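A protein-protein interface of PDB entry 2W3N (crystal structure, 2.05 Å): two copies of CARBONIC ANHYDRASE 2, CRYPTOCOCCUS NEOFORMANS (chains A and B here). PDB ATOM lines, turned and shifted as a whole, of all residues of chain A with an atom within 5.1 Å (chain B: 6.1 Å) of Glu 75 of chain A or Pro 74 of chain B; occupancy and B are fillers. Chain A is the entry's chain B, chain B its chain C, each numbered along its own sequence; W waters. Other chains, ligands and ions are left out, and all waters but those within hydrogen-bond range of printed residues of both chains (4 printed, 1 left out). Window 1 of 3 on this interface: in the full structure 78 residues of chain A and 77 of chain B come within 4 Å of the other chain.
The side-chain carboxylate (OE2) of Glu 75 of chain B is in salt-bridge range of the guanidinium group (NH1) of Arg 90 of chain A, 3.3 Å away. The side-chain carboxylate of Glu 75 of chain A is in salt-bridge range of the guanidinium group of Arg 90 of chain B (3.0 Å). N of Arg 90 of chain A sits at hydrogen-bond distance from O of Arg 90 of chain B.
O of Val 73 of chain A lies within hydrogen-bond range of NH2 of Arg 90 of chain A, 3.5 Å away. The side-chain carboxylate of Glu 75 of chain B is in salt-bridge range of the guanidinium group of Arg 90 of chain B, at 3.8 Å. The side-chain carboxylate (OD1) of Asp 70 of chain B is in salt-bridge range of the guanidinium group (NE) of Arg 72 of chain B. OE1 of Glu 75 of chain A is in salt-bridge range of NH1 of Arg 90 of chain A, 3.5 Å away. The guanidinium group of Arg 90 of chain B sits at hydrogen-bond distance from the backbone carbonyl oxygen of Asp 70 of chain B (2.7 Å).
Among the printed residues, merely in contact across the chains: Val 76 of chain A with Thr 77 of chain B, Val 86 of chain A with Ser 71 of chain B, Thr 77 of chain A with Val 76 of chain B, Val 88 of chain A with Arg 90 of chain B, Pro 83 of chain A with Ser 71 of chain B, Glu 75 of chain A with Pro 74 of chain B, Val 76 of chain A with Pro 74 of chain B, Pro 74 of chain A with Val 76 of chain B, Pro 83 of chain A with Thr 77 of chain B, Pro 83 of chain A with Pro 74 of chain B, Pro 83 of chain A with Arg 72 of chain B and Pro 74 of chain A with Glu 75 of chain B.
Of the printed residues of chain B, Glu 75 of chain A touches Pro 74 (3.7 Å) and Arg 90 (3.0 Å). Of the printed residues of chain B, Val 76 of chain A touches Pro 74 (3.7 Å) and Thr 77 (3.2 Å). Of the printed residues of chain B, Thr 77 of chain A touches Val 76 (3.3 Å). Of the printed residues of chain B, Val 88 of chain A touches Arg 90 (3.5 Å). Of the printed residues of chain B, Arg 90 of chain A touches Glu 75 (3.3 Å) and Arg 90 (3.3 Å). The nearest residue of chain B that does not touch Glu 75 of chain A is Glu 75 of chain B (4.8 Å). The nearest printed residue of chain B that does not touch Val 88 of chain A is Asp 70 of chain B (5.1 Å).
Hydrophobic or aromatic side chains of chain A within 4 Å of the printed part of chain B: Pro 74, Val 76, Pro 83 and Val 88. Of the 12 printed residues of chain B, 7 touch a printed residue of chain A.
Pro 74 of chain A touches Glu 75 of chain B, and with the chains exchanged Glu 75 of chain A touches Pro 74 of chain B. Pro 74 of chain A touches Val 76 of chain B, and with the chains exchanged Val 76 of chain A touches Pro 74 of chain B. Val 76 of chain A touches Thr 77 of chain B, and with the chains exchanged Thr 77 of chain A touches Val 76 of chain B. Arg 90 of chain A touches its own counterpart, Arg 90 of chain B.
Water W1 lies within hydrogen-bond range of the side-chain carboxylate of Glu 75 of chain A, the guanidinium group of Arg 90 of chain A, the side-chain carboxylate of Glu 75 of chain B and the guanidinium group of Arg 90 of chain B. Water W4 lies within hydrogen-bond range of OE2 of Glu 75 of chain B and OE2 of Glu 75 of chain A. Water W3 bridges the backbone carbonyl oxygen of Ser 71 of chain B and the backbone NH of Val 86 of chain A. Water W2 lies within hydrogen-bond range of the backbone carbonyl oxygen (O) of Arg 90 of chain B (2.9 Å) and the backbone carbonyl oxygen (O) of Arg 90 of chain A (3.0 Å).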
ATOM      1  N   TRP A  65      10.827  11.604  17.440  1.00  0.00           N
ATOM      2  CA  TRP A  65      11.499  12.787  16.990  1.00  0.00           C
ATOM      3  C   TRP A  65      12.887  12.367  16.542  1.00  0.00           C
ATOM      4  O   TRP A  65      13.684  11.889  17.346  1.00  0.00           O
ATOM      5  CB  TRP A  65      11.594  13.749  18.170  1.00  0.00           C
ATOM      6  CG  TRP A  65      12.391  15.026  18.007  1.00  0.00           C
ATOM      7  CD1 TRP A  65      13.721  15.179  18.108  1.00  0.00           C
ATOM      8  CD2 TRP A  65      11.847  16.357  17.876  1.00  0.00           C
ATOM      9  NE1 TRP A  65      14.064  16.509  17.971  1.00  0.00           N
ATOM     10  CE2 TRP A  65      12.921  17.246  17.840  1.00  0.00           C
ATOM     11  CE3 TRP A  65      10.551  16.864  17.764  1.00  0.00           C
ATOM     12  CZ2 TRP A  65      12.747  18.640  17.717  1.00  0.00           C
ATOM     13  CZ3 TRP A  65      10.385  18.254  17.646  1.00  0.00           C
ATOM     14  CH2 TRP A  65      11.487  19.104  17.604  1.00  0.00           C
ATOM     15  N   VAL A  73      17.816  22.828  20.519  1.00  0.00           N
ATOM     16  CA  VAL A  73      16.618  22.143  19.998  1.00  0.00           C
ATOM     17  C   VAL A  73      16.157  20.926  20.866  1.00  0.00           C
ATOM     18  O   VAL A  73      16.113  19.795  20.371  1.00  0.00           O
ATOM     19  CB  VAL A  73      16.831  21.778  18.501  1.00  0.00           C
ATOM     20  CG1 VAL A  73      15.481  21.583  17.763  1.00  0.00           C
ATOM     21  CG2 VAL A  73      17.616  22.890  17.804  1.00  0.00           C
ATOM     22  N   PRO A  74      15.818  21.157  22.160  1.00  0.00           N
ATOM     23  CA  PRO A  74      15.170  20.114  22.988  1.00  0.00           C
ATOM     24  C   PRO A  74      13.680  19.887  22.657  1.00  0.00           C
ATOM     25  O   PRO A  74      12.830  20.786  22.822  1.00  0.00           O
ATOM     26  CB  PRO A  74      15.317  20.650  24.411  1.00  0.00           C
ATOM     27  CG  PRO A  74      15.282  22.169  24.225  1.00  0.00           C
ATOM     28  CD  PRO A  74      16.029  22.405  22.923  1.00  0.00           C
ATOM     29  N   GLU A  75      13.369  18.669  22.248  1.00  0.00           N
ATOM     30  CA  GLU A  75      12.074  18.356  21.695  1.00  0.00           C
ATOM     31  C   GLU A  75      10.913  18.588  22.652  1.00  0.00           C
ATOM     32  O   GLU A  75       9.921  19.191  22.267  1.00  0.00           O
ATOM     33  CB  GLU A  75      12.073  16.925  21.136  1.00  0.00           C
ATOM     34  CG  GLU A  75      12.005  15.811  22.178  1.00  0.00           C
ATOM     35  CD  GLU A  75      13.253  15.762  23.032  1.00  0.00           C
ATOM     36  OE1 GLU A  75      14.343  16.126  22.502  1.00  0.00           O
ATOM     37  OE2 GLU A  75      13.142  15.403  24.237  1.00  0.00           O
ATOM     38  N   VAL A  76      11.024  18.139  23.901  1.00  0.00           N
ATOM     39  CA  VAL A  76       9.904  18.235  24.843  1.00  0.00           C
ATOM     40  C   VAL A  76       9.543  19.682  25.196  1.00  0.00           C
ATOM     41  O   VAL A  76       8.361  20.014  25.291  1.00  0.00           O
ATOM     42  CB  VAL A  76      10.148  17.401  26.117  1.00  0.00           C
ATOM     43  CG1 VAL A  76       9.279  17.847  27.242  1.00  0.00           C
ATOM     44  CG2 VAL A  76       9.839  15.908  25.822  1.00  0.00           C
ATOM     45  N   THR A  77      10.549  20.524  25.360  1.00  0.00           N
ATOM     46  CA  THR A  77      10.354  21.954  25.613  1.00  0.00           C
ATOM     47  C   THR A  77       9.698  22.637  24.428  1.00  0.00           C
ATOM     48  O   THR A  77       8.631  23.235  24.539  1.00  0.00           O
ATOM     49  CB  THR A  77      11.721  22.643  25.894  1.00  0.00           C
ATOM     50  OG1 THR A  77      12.365  21.994  27.007  1.00  0.00           O
ATOM     51  CG2 THR A  77      11.541  24.133  26.187  1.00  0.00           C
ATOM     52  N   ILE A  78      10.336  22.533  23.273  1.00  0.00           N
ATOM     53  CA  ILE A  78       9.835  23.246  22.135  1.00  0.00           C
ATOM     54  C   ILE A  78       8.463  22.732  21.592  1.00  0.00           C
ATOM     55  O   ILE A  78       7.750  23.486  20.938  1.00  0.00           O
ATOM     56  CB  ILE A  78      10.929  23.504  21.049  1.00  0.00           C
ATOM     57  CG1 ILE A  78      11.142  22.329  20.152  1.00  0.00           C
ATOM     58  CG2 ILE A  78      12.290  23.927  21.681  1.00  0.00           C
ATOM     59  CD1 ILE A  78      12.455  22.494  19.388  1.00  0.00           C
ATOM     60  N   MET A  79       8.095  21.480  21.875  1.00  0.00           N
ATOM     61  CA  MET A  79       6.751  20.995  21.549  1.00  0.00           C
ATOM     62  C   MET A  79       5.804  21.094  22.722  1.00  0.00           C
ATOM     63  O   MET A  79       4.685  20.604  22.652  1.00  0.00           O
ATOM     64  CB  MET A  79       6.787  19.553  21.113  1.00  0.00           C
ATOM     65  CG  MET A  79       7.469  19.328  19.798  1.00  0.00           C
ATOM     66  SD  MET A  79       6.983  17.682  19.248  1.00  0.00           S
ATOM     67  CE  MET A  79       8.212  16.654  19.994  1.00  0.00           C
ATOM     68  N   ALA A  80       6.273  21.714  23.792  1.00  0.00           N
ATOM     69  CA  ALA A  80       5.559  21.771  25.050  1.00  0.00           C
ATOM     70  C   ALA A  80       4.911  20.452  25.377  1.00  0.00           C
ATOM     71  O   ALA A  80       3.714  20.400  25.601  1.00  0.00           O
ATOM     72  CB  ALA A  80       4.518  22.897  25.040  1.00  0.00           C
ATOM     73  N   PRO A  83       7.468  14.209  29.704  1.00  0.00           N
ATOM     74  CA  PRO A  83       8.108  12.891  29.615  1.00  0.00           C
ATOM     75  C   PRO A  83       7.083  11.824  29.257  1.00  0.00           C
ATOM     76  O   PRO A  83       5.960  11.865  29.750  1.00  0.00           O
ATOM     77  CB  PRO A  83       8.671  12.686  31.015  1.00  0.00           C
ATOM     78  CG  PRO A  83       8.993  14.138  31.478  1.00  0.00           C
ATOM     79  CD  PRO A  83       7.836  14.928  30.943  1.00  0.00           C
ATOM     80  N   VAL A  86       7.326  11.538  23.632  1.00  0.00           N
ATOM     81  CA  VAL A  86       8.195  11.606  22.453  1.00  0.00           C
ATOM     82  C   VAL A  86       9.450  10.723  22.594  1.00  0.00           C
ATOM     83  O   VAL A  86      10.312  10.978  23.427  1.00  0.00           O
ATOM     84  CB  VAL A  86       8.692  13.034  22.144  1.00  0.00           C
ATOM     85  CG1 VAL A  86       9.370  13.064  20.748  1.00  0.00           C
ATOM     86  CG2 VAL A  86       7.553  14.030  22.172  1.00  0.00           C
ATOM     87  N   VAL A  88      12.986   9.488  21.102  1.00  0.00           N
ATOM     88  CA  VAL A  88      13.888  10.442  20.486  1.00  0.00           C
ATOM     89  C   VAL A  88      15.162   9.824  19.958  1.00  0.00           C
ATOM     90  O   VAL A  88      15.876   9.105  20.688  1.00  0.00           O
ATOM     91  CB  VAL A  88      14.291  11.565  21.469  1.00  0.00           C
ATOM     92  CG1 VAL A  88      15.297  12.539  20.831  1.00  0.00           C
ATOM     93  CG2 VAL A  88      13.051  12.324  21.959  1.00  0.00           C
ATOM     94  N   ARG A  90      18.703  11.687  18.566  1.00  0.00           N
ATOM     95  CA  ARG A  90      19.419  12.923  18.276  1.00  0.00           C
ATOM     96  C   ARG A  90      20.869  12.602  17.920  1.00  0.00           C
ATOM     97  O   ARG A  90      21.574  11.872  18.679  1.00  0.00           O
ATOM     98  CB  ARG A  90      19.333  13.879  19.459  1.00  0.00           C
ATOM     99  CG  ARG A  90      18.000  14.700  19.461  1.00  0.00           C
ATOM    100  CD  ARG A  90      17.786  15.487  20.769  1.00  0.00           C
ATOM    101  NE  ARG A  90      18.538  16.741  20.808  1.00  0.00           N
ATOM    102  CZ  ARG A  90      18.419  17.614  21.793  1.00  0.00           C
ATOM    103  NH1 ARG A  90      17.584  17.345  22.808  1.00  0.00           N
ATOM    104  NH2 ARG A  90      19.114  18.750  21.766  1.00  0.00           N
ATOM    105  N   TRP B  65      25.005  15.323  27.008  1.00  0.00           N
ATOM    106  CA  TRP B  65      24.220  14.229  27.570  1.00  0.00           C
ATOM    107  C   TRP B  65      24.234  13.062  26.600  1.00  0.00           C
ATOM    108  O   TRP B  65      23.834  13.187  25.431  1.00  0.00           O
ATOM    109  CB  TRP B  65      22.801  14.743  27.738  1.00  0.00           C
ATOM    110  CG  TRP B  65      21.762  13.819  28.216  1.00  0.00           C
ATOM    111  CD1 TRP B  65      21.078  12.872  27.474  1.00  0.00           C
ATOM    112  CD2 TRP B  65      21.186  13.804  29.527  1.00  0.00           C
ATOM    113  NE1 TRP B  65      20.125  12.257  28.268  1.00  0.00           N
ATOM    114  CE2 TRP B  65      20.170  12.810  29.529  1.00  0.00           C
ATOM    115  CE3 TRP B  65      21.440  14.531  30.718  1.00  0.00           C
ATOM    116  CZ2 TRP B  65      19.398  12.521  30.674  1.00  0.00           C
ATOM    117  CZ3 TRP B  65      20.684  14.254  31.856  1.00  0.00           C
ATOM    118  CH2 TRP B  65      19.666  13.250  31.834  1.00  0.00           C
ATOM    119  N   ASP B  70      14.464   6.532  25.013  1.00  0.00           N
ATOM    120  CA  ASP B  70      13.262   6.347  25.806  1.00  0.00           C
ATOM    121  C   ASP B  70      12.521   7.657  26.064  1.00  0.00           C
ATOM    122  O   ASP B  70      13.128   8.660  26.471  1.00  0.00           O
ATOM    123  CB  ASP B  70      13.641   5.740  27.150  1.00  0.00           C
ATOM    124  CG  ASP B  70      12.467   5.177  27.859  1.00  0.00           C
ATOM    125  OD1 ASP B  70      11.635   5.946  28.378  1.00  0.00           O
ATOM    126  OD2 ASP B  70      12.402   3.936  27.932  1.00  0.00           O
ATOM    127  N   SER B  71      11.207   7.633  25.864  1.00  0.00           N
ATOM    128  CA  SER B  71      10.445   8.871  25.869  1.00  0.00           C
ATOM    129  C   SER B  71      10.304   9.495  27.267  1.00  0.00           C
ATOM    130  O   SER B  71       9.922  10.687  27.390  1.00  0.00           O
ATOM    131  CB  SER B  71       9.065   8.642  25.275  1.00  0.00           C
ATOM    132  OG  SER B  71       8.268   7.866  26.135  1.00  0.00           O
ATOM    133  N   ARG B  72      10.590   8.693  28.297  1.00  0.00           N
ATOM    134  CA  ARG B  72      10.426   9.134  29.687  1.00  0.00           C
ATOM    135  C   ARG B  72      11.666   9.868  30.216  1.00  0.00           C
ATOM    136  O   ARG B  72      11.681  10.319  31.358  1.00  0.00           O
ATOM    137  CB  ARG B  72      10.056   7.935  30.609  1.00  0.00           C
ATOM    138  CG  ARG B  72       8.813   7.187  30.144  1.00  0.00           C
ATOM    139  CD  ARG B  72       8.664   5.823  30.792  1.00  0.00           C
ATOM    140  NE  ARG B  72       9.659   4.896  30.295  1.00  0.00           N
ATOM    141  CZ  ARG B  72       9.647   3.590  30.551  1.00  0.00           C
ATOM    142  NH1 ARG B  72       8.685   3.072  31.316  1.00  0.00           N
ATOM    143  NH2 ARG B  72      10.594   2.811  30.028  1.00  0.00           N
ATOM    144  N   VAL B  73      12.689  10.002  29.372  1.00  0.00           N
ATOM    145  CA  VAL B  73      13.984  10.573  29.760  1.00  0.00           C
ATOM    146  C   VAL B  73      14.484  11.799  28.896  1.00  0.00           C
ATOM    147  O   VAL B  73      15.635  11.813  28.403  1.00  0.00           O
ATOM    148  CB  VAL B  73      15.082   9.455  29.830  1.00  0.00           C
ATOM    149  CG1 VAL B  73      16.249   9.894  30.701  1.00  0.00           C
ATOM    150  CG2 VAL B  73      14.517   8.189  30.420  1.00  0.00           C
ATOM    151  N   PRO B  74      13.645  12.847  28.761  1.00  0.00           N
ATOM    152  CA  PRO B  74      14.091  14.135  28.143  1.00  0.00           C
ATOM    153  C   PRO B  74      14.971  14.961  29.121  1.00  0.00           C
ATOM    154  O   PRO B  74      14.502  15.411  30.185  1.00  0.00           O
ATOM    155  CB  PRO B  74      12.783  14.851  27.863  1.00  0.00           C
ATOM    156  CG  PRO B  74      11.859  14.380  28.984  1.00  0.00           C
ATOM    157  CD  PRO B  74      12.270  12.931  29.296  1.00  0.00           C
ATOM    158  N   GLU B  75      16.228  15.154  28.770  1.00  0.00           N
ATOM    159  CA  GLU B  75      17.231  15.736  29.663  1.00  0.00           C
ATOM    160  C   GLU B  75      16.894  17.129  30.221  1.00  0.00           C
ATOM    161  O   GLU B  75      17.055  17.387  31.419  1.00  0.00           O
ATOM    162  CB  GLU B  75      18.576  15.802  28.920  1.00  0.00           C
ATOM    163  CG  GLU B  75      18.679  16.824  27.792  1.00  0.00           C
ATOM    164  CD  GLU B  75      17.710  16.573  26.622  1.00  0.00           C
ATOM    165  OE1 GLU B  75      17.499  15.402  26.217  1.00  0.00           O
ATOM    166  OE2 GLU B  75      17.141  17.566  26.110  1.00  0.00           O
ATOM    167  N   VAL B  76      16.451  18.031  29.343  1.00  0.00           N
ATOM    168  CA  VAL B  76      16.156  19.419  29.701  1.00  0.00           C
ATOM    169  C   VAL B  76      15.005  19.517  30.716  1.00  0.00           C
ATOM    170  O   VAL B  76      15.027  20.346  31.616  1.00  0.00           O
ATOM    171  CB  VAL B  76      15.863  20.249  28.417  1.00  0.00           C
ATOM    172  CG1 VAL B  76      15.135  21.516  28.722  1.00  0.00           C
ATOM    173  CG2 VAL B  76      17.147  20.560  27.717  1.00  0.00           C
ATOM    174  N   THR B  77      14.014  18.646  30.578  1.00  0.00           N
ATOM    175  CA  THR B  77      12.863  18.641  31.480  1.00  0.00           C
ATOM    176  C   THR B  77      13.197  18.141  32.861  1.00  0.00           C
ATOM    177  O   THR B  77      12.796  18.742  33.863  1.00  0.00           O
ATOM    178  CB  THR B  77      11.780  17.716  30.947  1.00  0.00           C
ATOM    179  OG1 THR B  77      11.171  18.335  29.806  1.00  0.00           O
ATOM    180  CG2 THR B  77      10.723  17.478  32.003  1.00  0.00           C
ATOM    181  N   ILE B  78      13.904  17.011  32.911  1.00  0.00           N
ATOM    182  CA  ILE B  78      14.146  16.331  34.161  1.00  0.00           C
ATOM    183  C   ILE B  78      15.309  16.979  34.901  1.00  0.00           C
ATOM    184  O   ILE B  78      15.535  16.673  36.063  1.00  0.00           O
ATOM    185  CB  ILE B  78      14.407  14.796  33.990  1.00  0.00           C
ATOM    186  CG1 ILE B  78      15.780  14.519  33.378  1.00  0.00           C
ATOM    187  CG2 ILE B  78      13.322  14.142  33.180  1.00  0.00           C
ATOM    188  CD1 ILE B  78      15.968  13.043  33.068  1.00  0.00           C
ATOM    189  N   MET B  79      16.031  17.884  34.235  1.00  0.00           N
ATOM    190  CA  MET B  79      17.077  18.669  34.901  1.00  0.00           C
ATOM    191  C   MET B  79      16.724  20.138  35.037  1.00  0.00           C
ATOM    192  O   MET B  79      17.607  20.942  35.354  1.00  0.00           O
ATOM    193  CB  MET B  79      18.396  18.583  34.163  1.00  0.00           C
ATOM    194  CG  MET B  79      18.938  17.223  34.068  1.00  0.00           C
ATOM    195  SD  MET B  79      20.689  17.441  33.749  1.00  0.00           S
ATOM    196  CE  MET B  79      20.758  17.775  31.974  1.00  0.00           C
ATOM    197  N   ARG B  90      21.054  10.836  21.757  1.00  0.00           N
ATOM    198  CA  ARG B  90      20.088   9.886  22.249  1.00  0.00           C
ATOM    199  C   ARG B  90      20.039   8.759  21.241  1.00  0.00           C
ATOM    200  O   ARG B  90      19.866   9.011  20.047  1.00  0.00           O
ATOM    201  CB  ARG B  90      18.716  10.537  22.486  1.00  0.00           C
ATOM    202  CG  ARG B  90      18.679  11.196  23.910  1.00  0.00           C
ATOM    203  CD  ARG B  90      17.448  12.024  24.289  1.00  0.00           C
ATOM    204  NE  ARG B  90      16.308  11.193  24.718  1.00  0.00           N
ATOM    205  CZ  ARG B  90      15.095  11.678  24.966  1.00  0.00           C
ATOM    206  NH1 ARG B  90      14.858  12.991  24.866  1.00  0.00           N
ATOM    207  NH2 ARG B  90      14.116  10.861  25.325  1.00  0.00           N
HETATM  208  O   HOH W   1      16.324  15.165  23.703  1.00  0.00           O
HETATM  209  O   HOH W   2      21.897   8.978  17.945  1.00  0.00           O
HETATM  210  O   HOH W   3       8.784  12.889  26.025  1.00  0.00           O
HETATM  211  O   HOH W   4      14.488  17.173  25.871  1.00  0.00           O
